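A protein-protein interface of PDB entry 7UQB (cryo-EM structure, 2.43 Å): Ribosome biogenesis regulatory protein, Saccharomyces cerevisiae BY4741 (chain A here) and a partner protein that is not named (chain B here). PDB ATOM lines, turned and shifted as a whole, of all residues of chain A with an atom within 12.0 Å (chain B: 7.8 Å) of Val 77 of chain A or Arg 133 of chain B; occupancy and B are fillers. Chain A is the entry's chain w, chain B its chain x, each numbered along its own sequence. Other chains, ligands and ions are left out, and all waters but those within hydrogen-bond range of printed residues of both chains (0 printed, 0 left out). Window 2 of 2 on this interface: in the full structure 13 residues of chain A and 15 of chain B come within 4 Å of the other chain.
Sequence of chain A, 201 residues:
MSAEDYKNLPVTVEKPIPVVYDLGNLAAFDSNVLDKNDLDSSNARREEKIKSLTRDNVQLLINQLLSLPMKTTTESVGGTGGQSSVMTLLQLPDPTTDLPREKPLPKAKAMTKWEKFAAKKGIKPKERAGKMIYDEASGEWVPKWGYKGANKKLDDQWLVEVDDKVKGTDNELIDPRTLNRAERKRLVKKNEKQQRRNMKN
The backbone NH (N) of Asp 480 of chain B is in hydrogen-bond range of the backbone carbonyl oxygen (O) of Thr 74 of chain A.
OG of Ser 76 of chain A is in hydrogen-bond range of O of Asp 480 of chain B (2.9 Å).
N of Ser 85 of chain A is in hydrogen-bond range of O of Glu 75 of chain A.
O of Thr 513 of chain B lies within hydrogen-bond range of N of Thr 132 of chain B, at 3.3 Å.
OG1 of Thr 132 of chain B sits at hydrogen-bond distance from O of His 514 of chain B (2.8 Å).
The backbone carbonyl oxygen (O) of Arg 133 of chain B is in hydrogen-bond range of the backbone NH (N) of Thr 513 of chain B, 3.1 Å away.
The backbone carbonyl oxygen of His 514 of chain B sits at hydrogen-bond distance from the guanidinium group of Arg 133 of chain B (3.4 Å).
Val 479 of chain B touches Thr 74 of chain A.
CB of Ser 76 of chain A touches O of Thr 132 of chain B, 3.3 Å away.
Ser 76 of chain A touches Val 479 of chain B (OG to CG2, 3.3 Å).
OG of Ser 76 of chain A touches CD2 of Leu 481 of chain B (3.2 Å).
CB of Arg 133 of chain B touches CG2 of Val 77 of chain A, at 3.7 Å.
Ser 85 of chain A touches Val 479 of chain B (CB to CG2, 3.7 Å).
Of the printed residues of chain B, Val 77 of chain A touches Arg 133.
Arg 133 of chain B touches just one residue of chain A: Val 77.
No residue of chain A comes within 4 Å of Val 131 of chain B.
Of chain A, only Ser 76 comes within 4 Å of Thr 132 of chain B.
No residue of chain A comes within 4 Å of Ser 134 of chain B.
Trp 512 of chain B touches none of the printed residues of chain A.
Of the printed residues of chain B, Ser 76 of chain A touches Thr 132 (3.3 Å), Val 479 (3.3 Å), Asp 480 (2.9 Å) and Leu 481 (3.2 Å).
Printed residues of chain A within 4 Å of Leu 481 of chain B: Ser 76.
Printed residues of chain B within 4 Å of Ser 85 of chain A: Val 479 (3.7 Å).
Leu 511 of chain B touches none of the printed residues of chain A.
Ser 136 of chain B touches none of the printed residues of chain A.
The nearest printed residue of chain B that does not touch Thr 74 of chain A is Leu 481 of chain B (5.8 Å).
Of the 18 printed residues of chain B, 5 touch a printed residue of chain A.
Hydrophobic or aromatic side chains of chain B within 4 Å of the printed part of chain A: Val 479 and Leu 481.
Hydrophobic or aromatic side chains of chain A that line the printed part of chain B: Val 77.
Among the printed residues, no Asp or Glu carboxylate lies within 4 Å of a Lys or Arg side-chain nitrogen of the other chain.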
ATOM      1  N   THR A  73      -6.661   1.243  17.205  1.00  0.00           N
ATOM      2  CA  THR A  73      -7.156   2.125  18.250  1.00  0.00           C
ATOM      3  C   THR A  73      -8.629   2.412  18.003  1.00  0.00           C
ATOM      4  O   THR A  73      -9.141   2.223  16.897  1.00  0.00           O
ATOM      5  CB  THR A  73      -6.363   3.438  18.310  1.00  0.00           C
ATOM      6  OG1 THR A  73      -6.852   4.242  19.390  1.00  0.00           O
ATOM      7  CG2 THR A  73      -6.506   4.205  17.014  1.00  0.00           C
ATOM      8  N   THR A  74      -9.312   2.856  19.056  1.00  0.00           N
ATOM      9  CA  THR A  74     -10.709   3.246  18.958  1.00  0.00           C
ATOM     10  C   THR A  74     -10.914   4.752  19.044  1.00  0.00           C
ATOM     11  O   THR A  74     -12.059   5.208  18.976  1.00  0.00           O
ATOM     12  CB  THR A  74     -11.542   2.553  20.045  1.00  0.00           C
ATOM     13  OG1 THR A  74     -11.060   2.929  21.340  1.00  0.00           O
ATOM     14  CG2 THR A  74     -11.462   1.042  19.897  1.00  0.00           C
ATOM     15  N   GLU A  75      -9.850   5.535  19.189  1.00  0.00           N
ATOM     16  CA  GLU A  75      -9.994   6.982  19.243  1.00  0.00           C
ATOM     17  C   GLU A  75     -10.262   7.546  17.852  1.00  0.00           C
ATOM     18  O   GLU A  75      -9.895   6.954  16.834  1.00  0.00           O
ATOM     19  CB  GLU A  75      -8.751   7.633  19.850  1.00  0.00           C
ATOM     20  CG  GLU A  75      -7.475   7.430  19.061  1.00  0.00           C
ATOM     21  CD  GLU A  75      -6.256   7.984  19.776  1.00  0.00           C
ATOM     22  OE1 GLU A  75      -6.422   8.882  20.629  1.00  0.00           O
ATOM     23  OE2 GLU A  75      -5.133   7.517  19.490  1.00  0.00           O
ATOM     24  N   SER A  76     -10.913   8.702  17.822  1.00  0.00           N
ATOM     25  CA  SER A  76     -11.363   9.332  16.593  1.00  0.00           C
ATOM     26  C   SER A  76     -10.354  10.382  16.129  1.00  0.00           C
ATOM     27  O   SER A  76      -9.242  10.487  16.652  1.00  0.00           O
ATOM     28  CB  SER A  76     -12.746   9.946  16.806  1.00  0.00           C
ATOM     29  OG  SER A  76     -13.619   9.024  17.425  1.00  0.00           O
ATOM     30  N   VAL A  77     -10.749  11.170  15.130  1.00  0.00           N
ATOM     31  CA  VAL A  77      -9.916  12.245  14.602  1.00  0.00           C
ATOM     32  C   VAL A  77     -10.120  13.495  15.446  1.00  0.00           C
ATOM     33  O   VAL A  77     -11.075  13.585  16.225  1.00  0.00           O
ATOM     34  CB  VAL A  77     -10.233  12.523  13.122  1.00  0.00           C
ATOM     35  CG1 VAL A  77     -10.025  11.268  12.291  1.00  0.00           C
ATOM     36  CG2 VAL A  77     -11.655  13.037  12.975  1.00  0.00           C
ATOM     37  N   GLY A  78      -9.224  14.468  15.296  1.00  0.00           N
ATOM     38  CA  GLY A  78      -9.298  15.701  16.046  1.00  0.00           C
ATOM     39  C   GLY A  78      -8.550  15.694  17.360  1.00  0.00           C
ATOM     40  O   GLY A  78      -8.409  16.755  17.980  1.00  0.00           O
ATOM     41  N   GLY A  79      -8.067  14.535  17.806  1.00  0.00           N
ATOM     42  CA  GLY A  79      -7.243  14.437  18.988  1.00  0.00           C
ATOM     43  C   GLY A  79      -5.780  14.239  18.621  1.00  0.00           C
ATOM     44  O   GLY A  79      -5.417  14.025  17.467  1.00  0.00           O
ATOM     45  N   THR A  80      -4.934  14.326  19.642  1.00  0.00           N
ATOM     46  CA  THR A  80      -3.514  14.090  19.444  1.00  0.00           C
ATOM     47  C   THR A  80      -3.247  12.601  19.259  1.00  0.00           C
ATOM     48  O   THR A  80      -3.967  11.746  19.781  1.00  0.00           O
ATOM     49  CB  THR A  80      -2.707  14.622  20.629  1.00  0.00           C
ATOM     50  OG1 THR A  80      -2.945  13.802  21.780  1.00  0.00           O
ATOM     51  CG2 THR A  80      -3.114  16.054  20.943  1.00  0.00           C
ATOM     52  N   GLY A  81      -2.200  12.294  18.500  1.00  0.00           N
ATOM     53  CA  GLY A  81      -1.819  10.914  18.276  1.00  0.00           C
ATOM     54  C   GLY A  81      -1.637  10.562  16.814  1.00  0.00           C
ATOM     55  O   GLY A  81      -0.742   9.789  16.462  1.00  0.00           O
ATOM     56  N   GLY A  82      -2.481  11.121  15.955  1.00  0.00           N
ATOM     57  CA  GLY A  82      -2.422  10.875  14.525  1.00  0.00           C
ATOM     58  C   GLY A  82      -3.201   9.670  14.039  1.00  0.00           C
ATOM     59  O   GLY A  82      -3.859   9.737  12.999  1.00  0.00           O
ATOM     60  N   GLN A  83      -3.146   8.565  14.778  1.00  0.00           N
ATOM     61  CA  GLN A  83      -3.839   7.345  14.387  1.00  0.00           C
ATOM     62  C   GLN A  83      -5.276   7.389  14.896  1.00  0.00           C
ATOM     63  O   GLN A  83      -5.508   7.514  16.103  1.00  0.00           O
ATOM     64  CB  GLN A  83      -3.126   6.108  14.928  1.00  0.00           C
ATOM     65  CG  GLN A  83      -3.808   4.807  14.537  1.00  0.00           C
ATOM     66  CD  GLN A  83      -3.186   3.590  15.190  1.00  0.00           C
ATOM     67  OE1 GLN A  83      -2.323   3.707  16.059  1.00  0.00           O
ATOM     68  NE2 GLN A  83      -3.627   2.409  14.773  1.00  0.00           N
ATOM     69  N   SER A  84      -6.229   7.285  13.979  1.00  0.00           N
ATOM     70  CA  SER A  84      -7.637   7.212  14.320  1.00  0.00           C
ATOM     71  C   SER A  84      -8.113   5.765  14.211  1.00  0.00           C
ATOM     72  O   SER A  84      -7.328   4.846  13.966  1.00  0.00           O
ATOM     73  CB  SER A  84      -8.449   8.151  13.428  1.00  0.00           C
ATOM     74  OG  SER A  84      -8.380   7.758  12.070  1.00  0.00           O
ATOM     75  N   SER A  85      -9.422   5.564  14.384  1.00  0.00           N
ATOM     76  CA  SER A  85      -9.984   4.218  14.448  1.00  0.00           C
ATOM     77  C   SER A  85      -9.815   3.467  13.133  1.00  0.00           C
ATOM     78  O   SER A  85      -9.589   2.252  13.133  1.00  0.00           O
ATOM     79  CB  SER A  85     -11.461   4.293  14.831  1.00  0.00           C
ATOM     80  OG  SER A  85     -12.087   3.032  14.697  1.00  0.00           O
ATOM     81  N   VAL A  86      -9.927   4.169  12.003  1.00  0.00           N
ATOM     82  CA  VAL A  86      -9.848   3.515  10.704  1.00  0.00           C
ATOM     83  C   VAL A  86      -8.431   3.077  10.357  1.00  0.00           C
ATOM     84  O   VAL A  86      -8.252   2.189   9.518  1.00  0.00           O
ATOM     85  CB  VAL A  86     -10.405   4.445   9.612  1.00  0.00           C
ATOM     86  CG1 VAL A  86     -11.912   4.555   9.734  1.00  0.00           C
ATOM     87  CG2 VAL A  86      -9.760   5.816   9.715  1.00  0.00           C
ATOM     88  N   MET A  87      -7.417   3.677  10.975  1.00  0.00           N
ATOM     89  CA  MET A  87      -6.031   3.368  10.658  1.00  0.00           C
ATOM     90  C   MET A  87      -5.542   2.170  11.461  1.00  0.00           C
ATOM     91  O   MET A  87      -5.840   2.037  12.650  1.00  0.00           O
ATOM     92  CB  MET A  87      -5.132   4.571  10.941  1.00  0.00           C
ATOM     93  CG  MET A  87      -5.525   5.840  10.213  1.00  0.00           C
ATOM     94  SD  MET A  87      -4.408   7.200  10.588  1.00  0.00           S
ATOM     95  CE  MET A  87      -2.847   6.506  10.048  1.00  0.00           C
ATOM     96  N   THR A  88      -4.789   1.298  10.797  1.00  0.00           N
ATOM     97  CA  THR A  88      -4.072   0.204  11.438  1.00  0.00           C
ATOM     98  C   THR A  88      -2.593   0.375  11.135  1.00  0.00           C
ATOM     99  O   THR A  88      -2.215   0.543   9.972  1.00  0.00           O
ATOM    100  CB  THR A  88      -4.564  -1.157  10.939  1.00  0.00           C
ATOM    101  OG1 THR A  88      -5.985  -1.246  11.101  1.00  0.00           O
ATOM    102  CG2 THR A  88      -3.903  -2.277  11.719  1.00  0.00           C
ATOM    103  N   PRO B 130     -18.659   2.656   9.509  1.00  0.00           N
ATOM    104  CA  PRO B 130     -18.808   3.227  10.852  1.00  0.00           C
ATOM    105  C   PRO B 130     -18.646   4.737  10.833  1.00  0.00           C
ATOM    106  O   PRO B 130     -17.823   5.283  10.095  1.00  0.00           O
ATOM    107  CB  PRO B 130     -17.680   2.560  11.652  1.00  0.00           C
ATOM    108  CG  PRO B 130     -17.251   1.385  10.832  1.00  0.00           C
ATOM    109  CD  PRO B 130     -17.492   1.768   9.411  1.00  0.00           C
ATOM    110  N   VAL B 131     -19.444   5.415  11.658  1.00  0.00           N
ATOM    111  CA  VAL B 131     -19.241   6.841  11.864  1.00  0.00           C
ATOM    112  C   VAL B 131     -18.000   7.040  12.722  1.00  0.00           C
ATOM    113  O   VAL B 131     -17.723   6.259  13.642  1.00  0.00           O
ATOM    114  CB  VAL B 131     -20.488   7.488  12.495  1.00  0.00           C
ATOM    115  CG1 VAL B 131     -21.654   7.430  11.522  1.00  0.00           C
ATOM    116  CG2 VAL B 131     -20.859   6.807  13.801  1.00  0.00           C
ATOM    117  N   THR B 132     -17.217   8.064  12.397  1.00  0.00           N
ATOM    118  CA  THR B 132     -15.928   8.271  13.040  1.00  0.00           C
ATOM    119  C   THR B 132     -15.665   9.706  13.459  1.00  0.00           C
ATOM    120  O   THR B 132     -14.677   9.950  14.159  1.00  0.00           O
ATOM    121  CB  THR B 132     -14.789   7.816  12.116  1.00  0.00           C
ATOM    122  OG1 THR B 132     -15.054   8.258  10.778  1.00  0.00           O
ATOM    123  CG2 THR B 132     -14.656   6.303  12.130  1.00  0.00           C
ATOM    124  N   ARG B 133     -16.502  10.657  13.062  1.00  0.00           N
ATOM    125  CA  ARG B 133     -16.259  12.057  13.362  1.00  0.00           C
ATOM    126  C   ARG B 133     -17.587  12.792  13.368  1.00  0.00           C
ATOM    127  O   ARG B 133     -18.569  12.343  12.774  1.00  0.00           O
ATOM    128  CB  ARG B 133     -15.302  12.682  12.343  1.00  0.00           C
ATOM    129  CG  ARG B 133     -15.786  12.550  10.912  1.00  0.00           C
ATOM    130  CD  ARG B 133     -14.726  12.981   9.920  1.00  0.00           C
ATOM    131  NE  ARG B 133     -15.272  13.094   8.573  1.00  0.00           N
ATOM    132  CZ  ARG B 133     -15.866  14.181   8.101  1.00  0.00           C
ATOM    133  NH1 ARG B 133     -16.005  15.268   8.839  1.00  0.00           N
ATOM    134  NH2 ARG B 133     -16.334  14.174   6.857  1.00  0.00           N
ATOM    135  N   SER B 134     -17.605  13.936  14.041  1.00  0.00           N
ATOM    136  CA  SER B 134     -18.804  14.757  14.094  1.00  0.00           C
ATOM    137  C   SER B 134     -18.901  15.578  12.817  1.00  0.00           C
ATOM    138  O   SER B 134     -18.017  16.392  12.531  1.00  0.00           O
ATOM    139  CB  SER B 134     -18.786  15.666  15.319  1.00  0.00           C
ATOM    140  OG  SER B 134     -20.004  16.383  15.428  1.00  0.00           O
ATOM    141  N   SER B 135     -19.963  15.348  12.044  1.00  0.00           N
ATOM    142  CA  SER B 135     -20.207  16.177  10.870  1.00  0.00           C
ATOM    143  C   SER B 135     -20.423  17.627  11.275  1.00  0.00           C
ATOM    144  O   SER B 135     -19.836  18.542  10.685  1.00  0.00           O
ATOM    145  CB  SER B 135     -21.413  15.654  10.091  1.00  0.00           C
ATOM    146  OG  SER B 135     -21.335  14.255   9.910  1.00  0.00           O
ATOM    147  N   SER B 136     -21.235  17.854  12.307  1.00  0.00           N
ATOM    148  CA  SER B 136     -21.516  19.226  12.713  1.00  0.00           C
ATOM    149  C   SER B 136     -22.099  19.280  14.116  1.00  0.00           C
ATOM    150  O   SER B 136     -22.662  18.305  14.622  1.00  0.00           O
ATOM    151  CB  SER B 136     -22.469  19.918  11.735  1.00  0.00           C
ATOM    152  OG  SER B 136     -22.801  21.219  12.185  1.00  0.00           O
ATOM    153  N   GLN B 175     -26.514  20.603   7.325  1.00  0.00           N
ATOM    154  CA  GLN B 175     -26.457  20.689   8.785  1.00  0.00           C
ATOM    155  C   GLN B 175     -26.909  22.062   9.280  1.00  0.00           C
ATOM    156  O   GLN B 175     -26.236  22.724  10.072  1.00  0.00           O
ATOM    157  CB  GLN B 175     -25.059  20.346   9.300  1.00  0.00           C
ATOM    158  CG  GLN B 175     -24.577  18.966   8.892  1.00  0.00           C
ATOM    159  CD  GLN B 175     -23.464  19.017   7.869  1.00  0.00           C
ATOM    160  OE1 GLN B 175     -22.405  19.587   8.118  1.00  0.00           O
ATOM    161  NE2 GLN B 175     -23.702  18.423   6.706  1.00  0.00           N
ATOM    162  N   VAL B 479     -15.348   2.438  17.833  1.00  0.00           N
ATOM    163  CA  VAL B 479     -14.850   3.806  17.960  1.00  0.00           C
ATOM    164  C   VAL B 479     -15.608   4.519  19.075  1.00  0.00           C
ATOM    165  O   VAL B 479     -16.798   4.279  19.292  1.00  0.00           O
ATOM    166  CB  VAL B 479     -14.939   4.555  16.603  1.00  0.00           C
ATOM    167  CG1 VAL B 479     -16.366   4.667  16.127  1.00  0.00           C
ATOM    168  CG2 VAL B 479     -14.275   5.925  16.674  1.00  0.00           C
ATOM    169  N   ASP B 480     -14.901   5.382  19.797  1.00  0.00           N
ATOM    170  CA  ASP B 480     -15.455   6.164  20.896  1.00  0.00           C
ATOM    171  C   ASP B 480     -15.542   7.621  20.458  1.00  0.00           C
ATOM    172  O   ASP B 480     -14.528   8.218  20.083  1.00  0.00           O
ATOM    173  CB  ASP B 480     -14.585   6.022  22.144  1.00  0.00           C
ATOM    174  CG  ASP B 480     -15.149   6.762  23.339  1.00  0.00           C
ATOM    175  OD1 ASP B 480     -16.375   6.993  23.381  1.00  0.00           O
ATOM    176  OD2 ASP B 480     -14.359   7.118  24.238  1.00  0.00           O
ATOM    177  N   LEU B 481     -16.746   8.191  20.510  1.00  0.00           N
ATOM    178  CA  LEU B 481     -17.008   9.533  20.001  1.00  0.00           C
ATOM    179  C   LEU B 481     -17.353  10.473  21.148  1.00  0.00           C
ATOM    180  O   LEU B 481     -18.479  10.433  21.670  1.00  0.00           O
ATOM    181  CB  LEU B 481     -18.148   9.495  18.981  1.00  0.00           C
ATOM    182  CG  LEU B 481     -18.024   8.466  17.854  1.00  0.00           C
ATOM    183  CD1 LEU B 481     -19.291   8.413  17.025  1.00  0.00           C
ATOM    184  CD2 LEU B 481     -16.827   8.783  16.977  1.00  0.00           C
ATOM    185  N   PRO B 482     -16.413  11.305  21.606  1.00  0.00           N
ATOM    186  CA  PRO B 482     -16.773  12.397  22.515  1.00  0.00           C
ATOM    187  C   PRO B 482     -17.125  13.661  21.745  1.00  0.00           C
ATOM    188  O   PRO B 482     -17.057  13.680  20.514  1.00  0.00           O
ATOM    189  CB  PRO B 482     -15.506  12.576  23.356  1.00  0.00           C
ATOM    190  CG  PRO B 482     -14.410  12.214  22.414  1.00  0.00           C
ATOM    191  CD  PRO B 482     -14.953  11.120  21.522  1.00  0.00           C
ATOM    192  N   VAL B 500     -25.526   9.730  11.877  1.00  0.00           N
ATOM    193  CA  VAL B 500     -25.993   9.452  13.229  1.00  0.00           C
ATOM    194  C   VAL B 500     -26.256  10.787  13.907  1.00  0.00           C
ATOM    195  O   VAL B 500     -25.413  11.688  13.858  1.00  0.00           O
ATOM    196  CB  VAL B 500     -24.974   8.616  14.028  1.00  0.00           C
ATOM    197  CG1 VAL B 500     -25.330   8.589  15.503  1.00  0.00           C
ATOM    198  CG2 VAL B 500     -24.910   7.202  13.483  1.00  0.00           C
ATOM    199  N   ARG B 510     -25.699  17.070  17.479  1.00  0.00           N
ATOM    200  CA  ARG B 510     -24.470  16.591  16.866  1.00  0.00           C
ATOM    201  C   ARG B 510     -24.828  15.628  15.745  1.00  0.00           C
ATOM    202  O   ARG B 510     -25.545  14.646  15.966  1.00  0.00           O
ATOM    203  CB  ARG B 510     -23.562  15.905  17.888  1.00  0.00           C
ATOM    204  CG  ARG B 510     -23.039  16.826  18.970  1.00  0.00           C
ATOM    205  CD  ARG B 510     -22.285  17.985  18.389  1.00  0.00           C
ATOM    206  NE  ARG B 510     -20.899  17.663  18.079  1.00  0.00           N
ATOM    207  CZ  ARG B 510     -19.858  18.110  18.768  1.00  0.00           C
ATOM    208  NH1 ARG B 510     -20.011  18.904  19.814  1.00  0.00           N
ATOM    209  NH2 ARG B 510     -18.632  17.757  18.392  1.00  0.00           N
ATOM    210  N   LEU B 511     -24.336  15.918  14.547  1.00  0.00           N
ATOM    211  CA  LEU B 511     -24.421  15.005  13.418  1.00  0.00           C
ATOM    212  C   LEU B 511     -23.051  14.389  13.194  1.00  0.00           C
ATOM    213  O   LEU B 511     -22.045  15.110  13.153  1.00  0.00           O
ATOM    214  CB  LEU B 511     -24.901  15.721  12.154  1.00  0.00           C
ATOM    215  CG  LEU B 511     -26.406  15.962  12.049  1.00  0.00           C
ATOM    216  CD1 LEU B 511     -26.752  16.555  10.697  1.00  0.00           C
ATOM    217  CD2 LEU B 511     -27.169  14.669  12.277  1.00  0.00           C
ATOM    218  N   TRP B 512     -23.025  13.064  13.057  1.00  0.00           N
ATOM    219  CA  TRP B 512     -21.817  12.272  12.880  1.00  0.00           C
ATOM    220  C   TRP B 512     -21.919  11.488  11.582  1.00  0.00           C
ATOM    221  O   TRP B 512     -23.004  11.030  11.209  1.00  0.00           O
ATOM    222  CB  TRP B 512     -21.612  11.280  14.034  1.00  0.00           C
ATOM    223  CG  TRP B 512     -21.900  11.816  15.400  1.00  0.00           C
ATOM    224  CD1 TRP B 512     -23.127  12.018  15.961  1.00  0.00           C
ATOM    225  CD2 TRP B 512     -20.940  12.191  16.390  1.00  0.00           C
ATOM    226  NE1 TRP B 512     -22.990  12.512  17.231  1.00  0.00           N
ATOM    227  CE2 TRP B 512     -21.657  12.624  17.522  1.00  0.00           C
ATOM    228  CE3 TRP B 512     -19.544  12.205  16.431  1.00  0.00           C
ATOM    229  CZ2 TRP B 512     -21.025  13.070  18.677  1.00  0.00           C
ATOM    230  CZ3 TRP B 512     -18.920  12.652  17.577  1.00  0.00           C
ATOM    231  CH2 TRP B 512     -19.659  13.076  18.684  1.00  0.00           C
ATOM    232  N   THR B 513     -20.783  11.317  10.910  1.00  0.00           N
ATOM    233  CA  THR B 513     -20.723  10.514   9.698  1.00  0.00           C
ATOM    234  C   THR B 513     -19.325   9.924   9.578  1.00  0.00           C
ATOM    235  O   THR B 513     -18.403  10.308  10.301  1.00  0.00           O
ATOM    236  CB  THR B 513     -21.086  11.335   8.455  1.00  0.00           C
ATOM    237  OG1 THR B 513     -21.538  10.456   7.417  1.00  0.00           O
ATOM    238  CG2 THR B 513     -19.883  12.122   7.954  1.00  0.00           C
ATOM    239  N   HIS B 514     -19.185   8.961   8.670  1.00  0.00           N
ATOM    240  CA  HIS B 514     -17.897   8.332   8.390  1.00  0.00           C
ATOM    241  C   HIS B 514     -16.870   9.347   7.898  1.00  0.00           C
ATOM    242  O   HIS B 514     -15.989   9.766   8.649  1.00  0.00           O
ATOM    243  CB  HIS B 514     -18.063   7.218   7.354  1.00  0.00           C
ATOM    244  CG  HIS B 514     -16.776   6.572   6.947  1.00  0.00           C
ATOM    245  ND1 HIS B 514     -16.208   5.534   7.653  1.00  0.00           N
ATOM    246  CD2 HIS B 514     -15.947   6.815   5.904  1.00  0.00           C
ATOM    247  CE1 HIS B 514     -15.084   5.167   7.066  1.00  0.00           C
ATOM    248  NE2 HIS B 514     -14.903   5.928   6.001  1.00  0.00           N
